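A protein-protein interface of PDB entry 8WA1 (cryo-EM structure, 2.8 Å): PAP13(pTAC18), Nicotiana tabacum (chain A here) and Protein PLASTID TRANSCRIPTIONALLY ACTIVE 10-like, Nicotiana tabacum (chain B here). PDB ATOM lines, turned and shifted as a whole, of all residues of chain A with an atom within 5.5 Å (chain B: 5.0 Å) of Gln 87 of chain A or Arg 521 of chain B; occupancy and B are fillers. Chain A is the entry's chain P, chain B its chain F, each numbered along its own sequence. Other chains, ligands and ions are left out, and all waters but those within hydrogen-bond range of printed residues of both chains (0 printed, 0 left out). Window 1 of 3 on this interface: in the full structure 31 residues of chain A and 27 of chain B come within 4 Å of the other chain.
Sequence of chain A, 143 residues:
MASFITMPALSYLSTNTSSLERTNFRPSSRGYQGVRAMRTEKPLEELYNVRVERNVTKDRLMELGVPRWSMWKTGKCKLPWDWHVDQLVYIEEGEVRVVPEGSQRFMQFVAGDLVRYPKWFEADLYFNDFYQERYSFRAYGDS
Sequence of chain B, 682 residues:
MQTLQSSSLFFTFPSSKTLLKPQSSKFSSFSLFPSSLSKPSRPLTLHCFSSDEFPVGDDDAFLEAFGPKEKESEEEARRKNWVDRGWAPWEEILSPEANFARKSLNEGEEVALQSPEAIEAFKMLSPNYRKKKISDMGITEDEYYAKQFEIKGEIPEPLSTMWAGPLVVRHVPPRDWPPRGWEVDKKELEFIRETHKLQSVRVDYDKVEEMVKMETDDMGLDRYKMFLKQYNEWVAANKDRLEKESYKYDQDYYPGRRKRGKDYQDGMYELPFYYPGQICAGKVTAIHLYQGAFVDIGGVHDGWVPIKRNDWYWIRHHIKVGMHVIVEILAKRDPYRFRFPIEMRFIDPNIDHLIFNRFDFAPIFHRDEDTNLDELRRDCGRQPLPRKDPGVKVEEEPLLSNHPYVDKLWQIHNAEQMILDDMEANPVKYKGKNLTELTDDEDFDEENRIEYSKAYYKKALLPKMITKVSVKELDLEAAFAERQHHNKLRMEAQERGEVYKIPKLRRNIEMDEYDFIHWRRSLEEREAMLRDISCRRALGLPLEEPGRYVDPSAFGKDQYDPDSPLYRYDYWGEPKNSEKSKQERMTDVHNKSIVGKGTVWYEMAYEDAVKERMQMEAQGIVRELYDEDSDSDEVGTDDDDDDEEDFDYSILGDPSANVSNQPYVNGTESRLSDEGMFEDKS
N of Tyr 117 of chain A lies within hydrogen-bond range of O of Gln 87 of chain A. The backbone NH (N) of Glu 133 of chain A lies within hydrogen-bond range of the backbone carbonyl oxygen (O) of Trp 72 of chain A (2.8 Å). The backbone NH (N) of Leu 88 of chain A is in hydrogen-bond range of the backbone carbonyl oxygen (O) of Ser 136 of chain A, at 2.9 Å.
Hydrophobic or aromatic side chains of chain A that line the printed part of chain B: Trp 72, Leu 79, Trp 81, Val 85, Tyr 135 and Phe 137. Among the printed residues, 17 pairs touch across the chains. Among the printed residues, Asp or Glu carboxylates within 4 Å of a Lys or Arg side-chain nitrogen of the other chain: Glu 133 of chain A with Arg 521 of chain B (3.98 Å).
OE1 of Glu 525 of chain B lies within hydrogen-bond range of NE1 of Trp 81 of chain A (2.7 Å). The backbone NH (N) of Arg 521 of chain B lies within hydrogen-bond range of the side-chain hydroxyl (OH) of Tyr 135 of chain A (3.2 Å). OE2 of Glu 133 of chain A is in salt-bridge range of NE of Arg 521 of chain B, 3.98 Å away. The guanidinium group (NH1) of Arg 521 of chain B lies within hydrogen-bond range of the side-chain amide oxygen (OE1) of Gln 87 of chain A, at 3.0 Å.
Of the printed residues of chain B, Val 85 of chain A touches Glu 525 (3.9 Å). Of the printed residues of chain B, Gln 87 of chain A touches Arg 521. Tyr 117 of chain A touches none of the printed residues of chain B. Of the printed residues of chain B, Tyr 135 of chain A touches Ile 517 (3.9 Å), Arg 520 (3.7 Å), Arg 521 (3.2 Å) and Glu 524 (3.2 Å). Printed residues of chain B within 4 Å of Ser 136 of chain A: Glu 524. Printed residues of chain B within 4 Å of Phe 137 of chain A: Arg 521 (3.5 Å), Glu 524 (3.8 Å) and Glu 525 (3.1 Å). Of chain A, only Trp 81 (3.3 Å), Gln 87 (3.0 Å), Glu 133 (3.98 Å), Tyr 135 (3.2 Å) and Phe 137 (3.5 Å) come within 4 Å of Arg 521 of chain B. The nearest printed residue of chain A that does not touch Arg 521 of chain B is Leu 79 of chain A (4.2 Å). The nearest printed residue of chain B that does not touch Trp 72 of chain A is Arg 521 of chain B (4.2 Å).
His 518 of chain B touches Trp 72 of chain A (CD2 to NE1, 3.9 Å). Leu 79 of chain A touches His 518 of chain B (CD1 to NE2, 3.8 Å). CE2 of Trp 81 of chain A touches NH2 of Arg 521 of chain B (3.3 Å). CG2 of Val 85 of chain A touches O of Glu 525 of chain B, at 3.9 Å. Ile 517 of chain B touches Tyr 135 of chain A. Tyr 135 of chain A touches Arg 520 of chain B (OH to C, 3.7 Å). Tyr 135 of chain A touches Glu 524 of chain B (CE2 to OE1, 3.2 Å). Glu 524 of chain B touches Ser 136 of chain A. Phe 137 of chain A touches Arg 521 of chain B (CE2 to O, 3.5 Å). N of Phe 137 of chain A touches OE2 of Glu 524 of chain B, at 3.8 Å.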
ATOM      1  N   TRP A  72      -9.772  19.650  -5.925  1.00  0.00           N
ATOM      2  CA  TRP A  72     -10.690  20.729  -6.255  1.00  0.00           C
ATOM      3  C   TRP A  72     -10.879  21.607  -5.026  1.00  0.00           C
ATOM      4  O   TRP A  72     -10.907  21.121  -3.892  1.00  0.00           O
ATOM      5  CB  TRP A  72     -12.039  20.180  -6.739  1.00  0.00           C
ATOM      6  CG  TRP A  72     -12.973  21.217  -7.278  1.00  0.00           C
ATOM      7  CD1 TRP A  72     -12.845  21.905  -8.449  1.00  0.00           C
ATOM      8  CD2 TRP A  72     -14.194  21.667  -6.678  1.00  0.00           C
ATOM      9  NE1 TRP A  72     -13.905  22.764  -8.610  1.00  0.00           N
ATOM     10  CE2 TRP A  72     -14.747  22.637  -7.537  1.00  0.00           C
ATOM     11  CE3 TRP A  72     -14.868  21.349  -5.495  1.00  0.00           C
ATOM     12  CZ2 TRP A  72     -15.944  23.290  -7.252  1.00  0.00           C
ATOM     13  CZ3 TRP A  72     -16.055  21.999  -5.214  1.00  0.00           C
ATOM     14  CH2 TRP A  72     -16.580  22.958  -6.087  1.00  0.00           C
ATOM     15  N   LEU A  79     -22.910  25.824  -5.869  1.00  0.00           N
ATOM     16  CA  LEU A  79     -22.652  24.997  -7.037  1.00  0.00           C
ATOM     17  C   LEU A  79     -23.802  24.027  -7.256  1.00  0.00           C
ATOM     18  O   LEU A  79     -23.883  23.008  -6.556  1.00  0.00           O
ATOM     19  CB  LEU A  79     -21.341  24.232  -6.874  1.00  0.00           C
ATOM     20  CG  LEU A  79     -20.963  23.291  -8.020  1.00  0.00           C
ATOM     21  CD1 LEU A  79     -20.689  24.075  -9.295  1.00  0.00           C
ATOM     22  CD2 LEU A  79     -19.767  22.431  -7.641  1.00  0.00           C
ATOM     23  N   TRP A  81     -25.205  20.967  -9.107  1.00  0.00           N
ATOM     24  CA  TRP A  81     -24.566  19.889  -9.846  1.00  0.00           C
ATOM     25  C   TRP A  81     -25.474  18.670  -9.892  1.00  0.00           C
ATOM     26  O   TRP A  81     -26.158  18.343  -8.919  1.00  0.00           O
ATOM     27  CB  TRP A  81     -23.217  19.504  -9.228  1.00  0.00           C
ATOM     28  CG  TRP A  81     -22.347  18.715 -10.153  1.00  0.00           C
ATOM     29  CD1 TRP A  81     -22.270  17.356 -10.249  1.00  0.00           C
ATOM     30  CD2 TRP A  81     -21.430  19.239 -11.120  1.00  0.00           C
ATOM     31  NE1 TRP A  81     -21.358  17.001 -11.214  1.00  0.00           N
ATOM     32  CE2 TRP A  81     -20.829  18.141 -11.764  1.00  0.00           C
ATOM     33  CE3 TRP A  81     -21.058  20.531 -11.502  1.00  0.00           C
ATOM     34  CZ2 TRP A  81     -19.877  18.295 -12.770  1.00  0.00           C
ATOM     35  CZ3 TRP A  81     -20.113  20.682 -12.500  1.00  0.00           C
ATOM     36  CH2 TRP A  81     -19.533  19.570 -13.122  1.00  0.00           C
ATOM     37  N   TRP A  83     -25.194  14.615 -10.657  1.00  0.00           N
ATOM     38  CA  TRP A  83     -24.240  13.519 -10.736  1.00  0.00           C
ATOM     39  C   TRP A  83     -24.727  12.500 -11.756  1.00  0.00           C
ATOM     40  O   TRP A  83     -25.688  11.768 -11.498  1.00  0.00           O
ATOM     41  CB  TRP A  83     -24.053  12.857  -9.373  1.00  0.00           C
ATOM     42  CG  TRP A  83     -23.128  13.594  -8.465  1.00  0.00           C
ATOM     43  CD1 TRP A  83     -21.795  13.367  -8.297  1.00  0.00           C
ATOM     44  CD2 TRP A  83     -23.465  14.676  -7.590  1.00  0.00           C
ATOM     45  NE1 TRP A  83     -21.279  14.240  -7.371  1.00  0.00           N
ATOM     46  CE2 TRP A  83     -22.284  15.054  -6.923  1.00  0.00           C
ATOM     47  CE3 TRP A  83     -24.650  15.361  -7.306  1.00  0.00           C
ATOM     48  CZ2 TRP A  83     -22.253  16.087  -5.990  1.00  0.00           C
ATOM     49  CZ3 TRP A  83     -24.617  16.386  -6.380  1.00  0.00           C
ATOM     50  CH2 TRP A  83     -23.427  16.738  -5.733  1.00  0.00           C
ATOM     51  N   VAL A  85     -22.695  10.134 -12.604  1.00  0.00           N
ATOM     52  CA  VAL A  85     -21.993   8.942 -12.146  1.00  0.00           C
ATOM     53  C   VAL A  85     -21.722   9.103 -10.660  1.00  0.00           C
ATOM     54  O   VAL A  85     -21.845  10.195 -10.099  1.00  0.00           O
ATOM     55  CB  VAL A  85     -20.663   8.695 -12.899  1.00  0.00           C
ATOM     56  CG1 VAL A  85     -20.920   8.080 -14.258  1.00  0.00           C
ATOM     57  CG2 VAL A  85     -19.878   9.993 -13.033  1.00  0.00           C
ATOM     58  N   ASP A  86     -21.351   8.001 -10.016  1.00  0.00           N
ATOM     59  CA  ASP A  86     -20.982   8.055  -8.612  1.00  0.00           C
ATOM     60  C   ASP A  86     -19.645   8.771  -8.445  1.00  0.00           C
ATOM     61  O   ASP A  86     -18.738   8.645  -9.270  1.00  0.00           O
ATOM     62  CB  ASP A  86     -20.905   6.646  -8.026  1.00  0.00           C
ATOM     63  CG  ASP A  86     -22.203   5.880  -8.184  1.00  0.00           C
ATOM     64  OD1 ASP A  86     -23.277   6.514  -8.129  1.00  0.00           O
ATOM     65  OD2 ASP A  86     -22.149   4.645  -8.365  1.00  0.00           O
ATOM     66  N   GLN A  87     -19.532   9.531  -7.359  1.00  0.00           N
ATOM     67  CA  GLN A  87     -18.351  10.338  -7.088  1.00  0.00           C
ATOM     68  C   GLN A  87     -17.952  10.170  -5.632  1.00  0.00           C
ATOM     69  O   GLN A  87     -18.768  10.396  -4.732  1.00  0.00           O
ATOM     70  CB  GLN A  87     -18.610  11.817  -7.396  1.00  0.00           C
ATOM     71  CG  GLN A  87     -17.430  12.732  -7.114  1.00  0.00           C
ATOM     72  CD  GLN A  87     -17.796  14.200  -7.221  1.00  0.00           C
ATOM     73  OE1 GLN A  87     -18.968  14.551  -7.340  1.00  0.00           O
ATOM     74  NE2 GLN A  87     -16.790  15.066  -7.181  1.00  0.00           N
ATOM     75  N   LEU A  88     -16.700   9.783  -5.404  1.00  0.00           N
ATOM     76  CA  LEU A  88     -16.146   9.635  -4.064  1.00  0.00           C
ATOM     77  C   LEU A  88     -15.336  10.884  -3.745  1.00  0.00           C
ATOM     78  O   LEU A  88     -14.370  11.197  -4.448  1.00  0.00           O
ATOM     79  CB  LEU A  88     -15.277   8.380  -3.957  1.00  0.00           C
ATOM     80  CG  LEU A  88     -15.977   7.036  -3.728  1.00  0.00           C
ATOM     81  CD1 LEU A  88     -16.768   6.596  -4.950  1.00  0.00           C
ATOM     82  CD2 LEU A  88     -14.965   5.972  -3.328  1.00  0.00           C
ATOM     83  N   VAL A  89     -15.729  11.589  -2.687  1.00  0.00           N
ATOM     84  CA  VAL A  89     -15.146  12.877  -2.336  1.00  0.00           C
ATOM     85  C   VAL A  89     -14.583  12.794  -0.926  1.00  0.00           C
ATOM     86  O   VAL A  89     -15.297  12.420   0.011  1.00  0.00           O
ATOM     87  CB  VAL A  89     -16.179  14.016  -2.432  1.00  0.00           C
ATOM     88  CG1 VAL A  89     -15.627  15.287  -1.812  1.00  0.00           C
ATOM     89  CG2 VAL A  89     -16.573  14.253  -3.880  1.00  0.00           C
ATOM     90  N   VAL A 115     -17.464  11.055   1.546  1.00  0.00           N
ATOM     91  CA  VAL A 115     -18.847  11.074   1.081  1.00  0.00           C
ATOM     92  C   VAL A 115     -18.885  10.597  -0.362  1.00  0.00           C
ATOM     93  O   VAL A 115     -18.134  11.096  -1.208  1.00  0.00           O
ATOM     94  CB  VAL A 115     -19.464  12.479   1.206  1.00  0.00           C
ATOM     95  CG1 VAL A 115     -20.961  12.428   0.944  1.00  0.00           C
ATOM     96  CG2 VAL A 115     -19.171  13.068   2.576  1.00  0.00           C
ATOM     97  N   ARG A 116     -19.754   9.628  -0.638  1.00  0.00           N
ATOM     98  CA  ARG A 116     -19.992   9.139  -1.989  1.00  0.00           C
ATOM     99  C   ARG A 116     -21.368   9.606  -2.446  1.00  0.00           C
ATOM    100  O   ARG A 116     -22.378   9.293  -1.804  1.00  0.00           O
ATOM    101  CB  ARG A 116     -19.892   7.615  -2.047  1.00  0.00           C
ATOM    102  CG  ARG A 116     -20.148   7.030  -3.427  1.00  0.00           C
ATOM    103  CD  ARG A 116     -19.945   5.521  -3.438  1.00  0.00           C
ATOM    104  NE  ARG A 116     -20.040   4.964  -4.785  1.00  0.00           N
ATOM    105  CZ  ARG A 116     -19.806   3.690  -5.086  1.00  0.00           C
ATOM    106  NH1 ARG A 116     -19.459   2.834  -4.135  1.00  0.00           N
ATOM    107  NH2 ARG A 116     -19.916   3.272  -6.339  1.00  0.00           N
ATOM    108  N   TYR A 117     -21.407  10.352  -3.551  1.00  0.00           N
ATOM    109  CA  TYR A 117     -22.671  10.870  -4.064  1.00  0.00           C
ATOM    110  C   TYR A 117     -23.287   9.880  -5.037  1.00  0.00           C
ATOM    111  O   TYR A 117     -22.590   9.387  -5.936  1.00  0.00           O
ATOM    112  CB  TYR A 117     -22.459  12.214  -4.754  1.00  0.00           C
ATOM    113  CG  TYR A 117     -22.102  13.333  -3.803  1.00  0.00           C
ATOM    114  CD1 TYR A 117     -20.779  13.599  -3.476  1.00  0.00           C
ATOM    115  CD2 TYR A 117     -23.091  14.122  -3.228  1.00  0.00           C
ATOM    116  CE1 TYR A 117     -20.450  14.621  -2.604  1.00  0.00           C
ATOM    117  CE2 TYR A 117     -22.770  15.146  -2.356  1.00  0.00           C
ATOM    118  CZ  TYR A 117     -21.449  15.391  -2.048  1.00  0.00           C
ATOM    119  OH  TYR A 117     -21.128  16.409  -1.181  1.00  0.00           O
ATOM    120  N   GLU A 133     -11.167  19.574  -1.588  1.00  0.00           N
ATOM    121  CA  GLU A 133     -11.606  18.188  -1.639  1.00  0.00           C
ATOM    122  C   GLU A 133     -10.777  17.421  -2.659  1.00  0.00           C
ATOM    123  O   GLU A 133     -10.121  18.003  -3.528  1.00  0.00           O
ATOM    124  CB  GLU A 133     -13.093  18.085  -2.002  1.00  0.00           C
ATOM    125  CG  GLU A 133     -13.403  18.525  -3.425  1.00  0.00           C
ATOM    126  CD  GLU A 133     -14.850  18.295  -3.814  1.00  0.00           C
ATOM    127  OE1 GLU A 133     -15.717  18.295  -2.915  1.00  0.00           O
ATOM    128  OE2 GLU A 133     -15.120  18.111  -5.018  1.00  0.00           O
ATOM    129  N   TYR A 135     -11.579  14.416  -5.376  1.00  0.00           N
ATOM    130  CA  TYR A 135     -12.731  13.798  -6.013  1.00  0.00           C
ATOM    131  C   TYR A 135     -12.289  12.710  -6.981  1.00  0.00           C
ATOM    132  O   TYR A 135     -11.287  12.861  -7.687  1.00  0.00           O
ATOM    133  CB  TYR A 135     -13.568  14.843  -6.757  1.00  0.00           C
ATOM    134  CG  TYR A 135     -12.821  15.552  -7.865  1.00  0.00           C
ATOM    135  CD1 TYR A 135     -12.041  16.669  -7.598  1.00  0.00           C
ATOM    136  CD2 TYR A 135     -12.899  15.107  -9.178  1.00  0.00           C
ATOM    137  CE1 TYR A 135     -11.356  17.319  -8.608  1.00  0.00           C
ATOM    138  CE2 TYR A 135     -12.218  15.750 -10.193  1.00  0.00           C
ATOM    139  CZ  TYR A 135     -11.449  16.857  -9.902  1.00  0.00           C
ATOM    140  OH  TYR A 135     -10.769  17.503 -10.909  1.00  0.00           O
ATOM    141  N   SER A 136     -13.046  11.615  -7.008  1.00  0.00           N
ATOM    142  CA  SER A 136     -12.830  10.529  -7.954  1.00  0.00           C
ATOM    143  C   SER A 136     -14.178  10.021  -8.440  1.00  0.00           C
ATOM    144  O   SER A 136     -14.963   9.488  -7.650  1.00  0.00           O
ATOM    145  CB  SER A 136     -12.028   9.389  -7.317  1.00  0.00           C
ATOM    146  OG  SER A 136     -11.921   8.288  -8.203  1.00  0.00           O
ATOM    147  N   PHE A 137     -14.445  10.183  -9.733  1.00  0.00           N
ATOM    148  CA  PHE A 137     -15.675   9.700 -10.343  1.00  0.00           C
ATOM    149  C   PHE A 137     -15.496   8.246 -10.755  1.00  0.00           C
ATOM    150  O   PHE A 137     -14.634   7.932 -11.582  1.00  0.00           O
ATOM    151  CB  PHE A 137     -16.061  10.545 -11.558  1.00  0.00           C
ATOM    152  CG  PHE A 137     -16.394  11.972 -11.227  1.00  0.00           C
ATOM    153  CD1 PHE A 137     -17.675  12.328 -10.839  1.00  0.00           C
ATOM    154  CD2 PHE A 137     -15.427  12.961 -11.316  1.00  0.00           C
ATOM    155  CE1 PHE A 137     -17.985  13.643 -10.539  1.00  0.00           C
ATOM    156  CE2 PHE A 137     -15.731  14.276 -11.016  1.00  0.00           C
ATOM    157  CZ  PHE A 137     -17.011  14.617 -10.627  1.00  0.00           C
ATOM    158  N   ARG A 138     -16.311   7.365 -10.181  1.00  0.00           N
ATOM    159  CA  ARG A 138     -16.224   5.933 -10.425  1.00  0.00           C
ATOM    160  C   ARG A 138     -17.443   5.451 -11.201  1.00  0.00           C
ATOM    161  O   ARG A 138     -18.551   5.969 -11.026  1.00  0.00           O
ATOM    162  CB  ARG A 138     -16.107   5.153  -9.112  1.00  0.00           C
ATOM    163  CG  ARG A 138     -14.849   5.452  -8.310  1.00  0.00           C
ATOM    164  CD  ARG A 138     -14.716   4.494  -7.134  1.00  0.00           C
ATOM    165  NE  ARG A 138     -13.506   4.739  -6.355  1.00  0.00           N
ATOM    166  CZ  ARG A 138     -12.310   4.246  -6.660  1.00  0.00           C
ATOM    167  NH1 ARG A 138     -12.161   3.480  -7.732  1.00  0.00           N
ATOM    168  NH2 ARG A 138     -11.262   4.520  -5.895  1.00  0.00           N
ATOM    169  N   ILE B 517      -9.439  23.935 -12.990  1.00  0.00           N
ATOM    170  CA  ILE B 517      -9.698  22.788 -12.122  1.00  0.00           C
ATOM    171  C   ILE B 517     -11.154  22.349 -12.246  1.00  0.00           C
ATOM    172  O   ILE B 517     -11.463  21.150 -12.185  1.00  0.00           O
ATOM    173  CB  ILE B 517      -9.305  23.094 -10.662  1.00  0.00           C
ATOM    174  CG1 ILE B 517     -10.171  24.203 -10.066  1.00  0.00           C
ATOM    175  CG2 ILE B 517      -7.829  23.457 -10.574  1.00  0.00           C
ATOM    176  CD1 ILE B 517      -9.809  24.567  -8.643  1.00  0.00           C
ATOM    177  N   HIS B 518     -12.068  23.302 -12.455  1.00  0.00           N
ATOM    178  CA  HIS B 518     -13.458  22.929 -12.700  1.00  0.00           C
ATOM    179  C   HIS B 518     -13.598  22.170 -14.017  1.00  0.00           C
ATOM    180  O   HIS B 518     -14.356  21.194 -14.105  1.00  0.00           O
ATOM    181  CB  HIS B 518     -14.343  24.174 -12.694  1.00  0.00           C
ATOM    182  CG  HIS B 518     -15.797  23.881 -12.495  1.00  0.00           C
ATOM    183  ND1 HIS B 518     -16.663  23.662 -13.545  1.00  0.00           N
ATOM    184  CD2 HIS B 518     -16.538  23.770 -11.368  1.00  0.00           C
ATOM    185  CE1 HIS B 518     -17.874  23.429 -13.073  1.00  0.00           C
ATOM    186  NE2 HIS B 518     -17.826  23.489 -11.755  1.00  0.00           N
ATOM    187  N   TRP B 519     -12.862  22.596 -15.046  1.00  0.00           N
ATOM    188  CA  TRP B 519     -12.877  21.882 -16.318  1.00  0.00           C
ATOM    189  C   TRP B 519     -12.286  20.485 -16.171  1.00  0.00           C
ATOM    190  O   TRP B 519     -12.772  19.533 -16.790  1.00  0.00           O
ATOM    191  CB  TRP B 519     -12.118  22.679 -17.378  1.00  0.00           C
ATOM    192  CG  TRP B 519     -11.955  21.945 -18.672  1.00  0.00           C
ATOM    193  CD1 TRP B 519     -12.804  21.964 -19.740  1.00  0.00           C
ATOM    194  CD2 TRP B 519     -10.876  21.077 -19.034  1.00  0.00           C
ATOM    195  NE1 TRP B 519     -12.319  21.164 -20.745  1.00  0.00           N
ATOM    196  CE2 TRP B 519     -11.137  20.607 -20.336  1.00  0.00           C
ATOM    197  CE3 TRP B 519      -9.714  20.651 -18.383  1.00  0.00           C
ATOM    198  CZ2 TRP B 519     -10.279  19.733 -20.999  1.00  0.00           C
ATOM    199  CZ3 TRP B 519      -8.865  19.785 -19.043  1.00  0.00           C
ATOM    200  CH2 TRP B 519      -9.151  19.334 -20.337  1.00  0.00           C
ATOM    201  N   ARG B 520     -11.232  20.346 -15.364  1.00  0.00           N
ATOM    202  CA  ARG B 520     -10.673  19.022 -15.100  1.00  0.00           C
ATOM    203  C   ARG B 520     -11.692  18.125 -14.409  1.00  0.00           C
ATOM    204  O   ARG B 520     -11.826  16.943 -14.752  1.00  0.00           O
ATOM    205  CB  ARG B 520      -9.409  19.133 -14.246  1.00  0.00           C
ATOM    206  CG  ARG B 520      -8.194  19.698 -14.958  1.00  0.00           C
ATOM    207  CD  ARG B 520      -6.920  19.228 -14.272  1.00  0.00           C
ATOM    208  NE  ARG B 520      -7.010  19.350 -12.819  1.00  0.00           N
ATOM    209  CZ  ARG B 520      -6.144  18.810 -11.967  1.00  0.00           C
ATOM    210  NH1 ARG B 520      -6.307  18.973 -10.661  1.00  0.00           N
ATOM    211  NH2 ARG B 520      -5.118  18.101 -12.420  1.00  0.00           N
ATOM    212  N   ARG B 521     -12.410  18.668 -13.423  1.00  0.00           N
ATOM    213  CA  ARG B 521     -13.442  17.892 -12.741  1.00  0.00           C
ATOM    214  C   ARG B 521     -14.523  17.443 -13.716  1.00  0.00           C
ATOM    215  O   ARG B 521     -14.937  16.277 -13.712  1.00  0.00           O
ATOM    216  CB  ARG B 521     -14.048  18.715 -11.602  1.00  0.00           C
ATOM    217  CG  ARG B 521     -15.098  17.973 -10.791  1.00  0.00           C
ATOM    218  CD  ARG B 521     -15.579  18.812  -9.616  1.00  0.00           C
ATOM    219  NE  ARG B 521     -16.494  18.072  -8.750  1.00  0.00           N
ATOM    220  CZ  ARG B 521     -17.818  18.172  -8.799  1.00  0.00           C
ATOM    221  NH1 ARG B 521     -18.568  17.459  -7.970  1.00  0.00           N
ATOM    222  NH2 ARG B 521     -18.393  18.987  -9.673  1.00  0.00           N
ATOM    223  N   SER B 522     -14.990  18.361 -14.567  1.00  0.00           N
ATOM    224  CA  SER B 522     -16.020  18.011 -15.542  1.00  0.00           C
ATOM    225  C   SER B 522     -15.517  16.968 -16.534  1.00  0.00           C
ATOM    226  O   SER B 522     -16.255  16.045 -16.905  1.00  0.00           O
ATOM    227  CB  SER B 522     -16.494  19.263 -16.277  1.00  0.00           C
ATOM    228  OG  SER B 522     -17.422  18.935 -17.295  1.00  0.00           O
ATOM    229  N   LEU B 523     -14.263  17.097 -16.975  1.00  0.00           N
ATOM    230  CA  LEU B 523     -13.698  16.134 -17.912  1.00  0.00           C
ATOM    231  C   LEU B 523     -13.591  14.754 -17.282  1.00  0.00           C
ATOM    232  O   LEU B 523     -13.893  13.745 -17.929  1.00  0.00           O
ATOM    233  CB  LEU B 523     -12.327  16.610 -18.393  1.00  0.00           C
ATOM    234  CG  LEU B 523     -11.576  15.652 -19.322  1.00  0.00           C
ATOM    235  CD1 LEU B 523     -12.268  15.558 -20.675  1.00  0.00           C
ATOM    236  CD2 LEU B 523     -10.124  16.075 -19.482  1.00  0.00           C
ATOM    237  N   GLU B 524     -13.159  14.686 -16.021  1.00  0.00           N
ATOM    238  CA  GLU B 524     -13.076  13.397 -15.343  1.00  0.00           C
ATOM    239  C   GLU B 524     -14.461  12.790 -15.158  1.00  0.00           C
ATOM    240  O   GLU B 524     -14.648  11.578 -15.321  1.00  0.00           O
ATOM    241  CB  GLU B 524     -12.366  13.557 -13.998  1.00  0.00           C
ATOM    242  CG  GLU B 524     -12.101  12.247 -13.279  1.00  0.00           C
ATOM    243  CD  GLU B 524     -11.259  12.424 -12.032  1.00  0.00           C
ATOM    244  OE1 GLU B 524     -10.704  13.526 -11.838  1.00  0.00           O
ATOM    245  OE2 GLU B 524     -11.152  11.461 -11.244  1.00  0.00           O
ATOM    246  N   GLU B 525     -15.450  13.624 -14.826  1.00  0.00           N
ATOM    247  CA  GLU B 525     -16.822  13.144 -14.700  1.00  0.00           C
ATOM    248  C   GLU B 525     -17.315  12.543 -16.012  1.00  0.00           C
ATOM    249  O   GLU B 525     -17.884  11.449 -16.033  1.00  0.00           O
ATOM    250  CB  GLU B 525     -17.743  14.278 -14.244  1.00  0.00           C
ATOM    251  CG  GLU B 525     -19.224  13.961 -14.402  1.00  0.00           C
ATOM    252  CD  GLU B 525     -20.120  14.935 -13.662  1.00  0.00           C
ATOM    253  OE1 GLU B 525     -19.800  15.276 -12.506  1.00  0.00           O
ATOM    254  OE2 GLU B 525     -21.146  15.359 -14.237  1.00  0.00           O
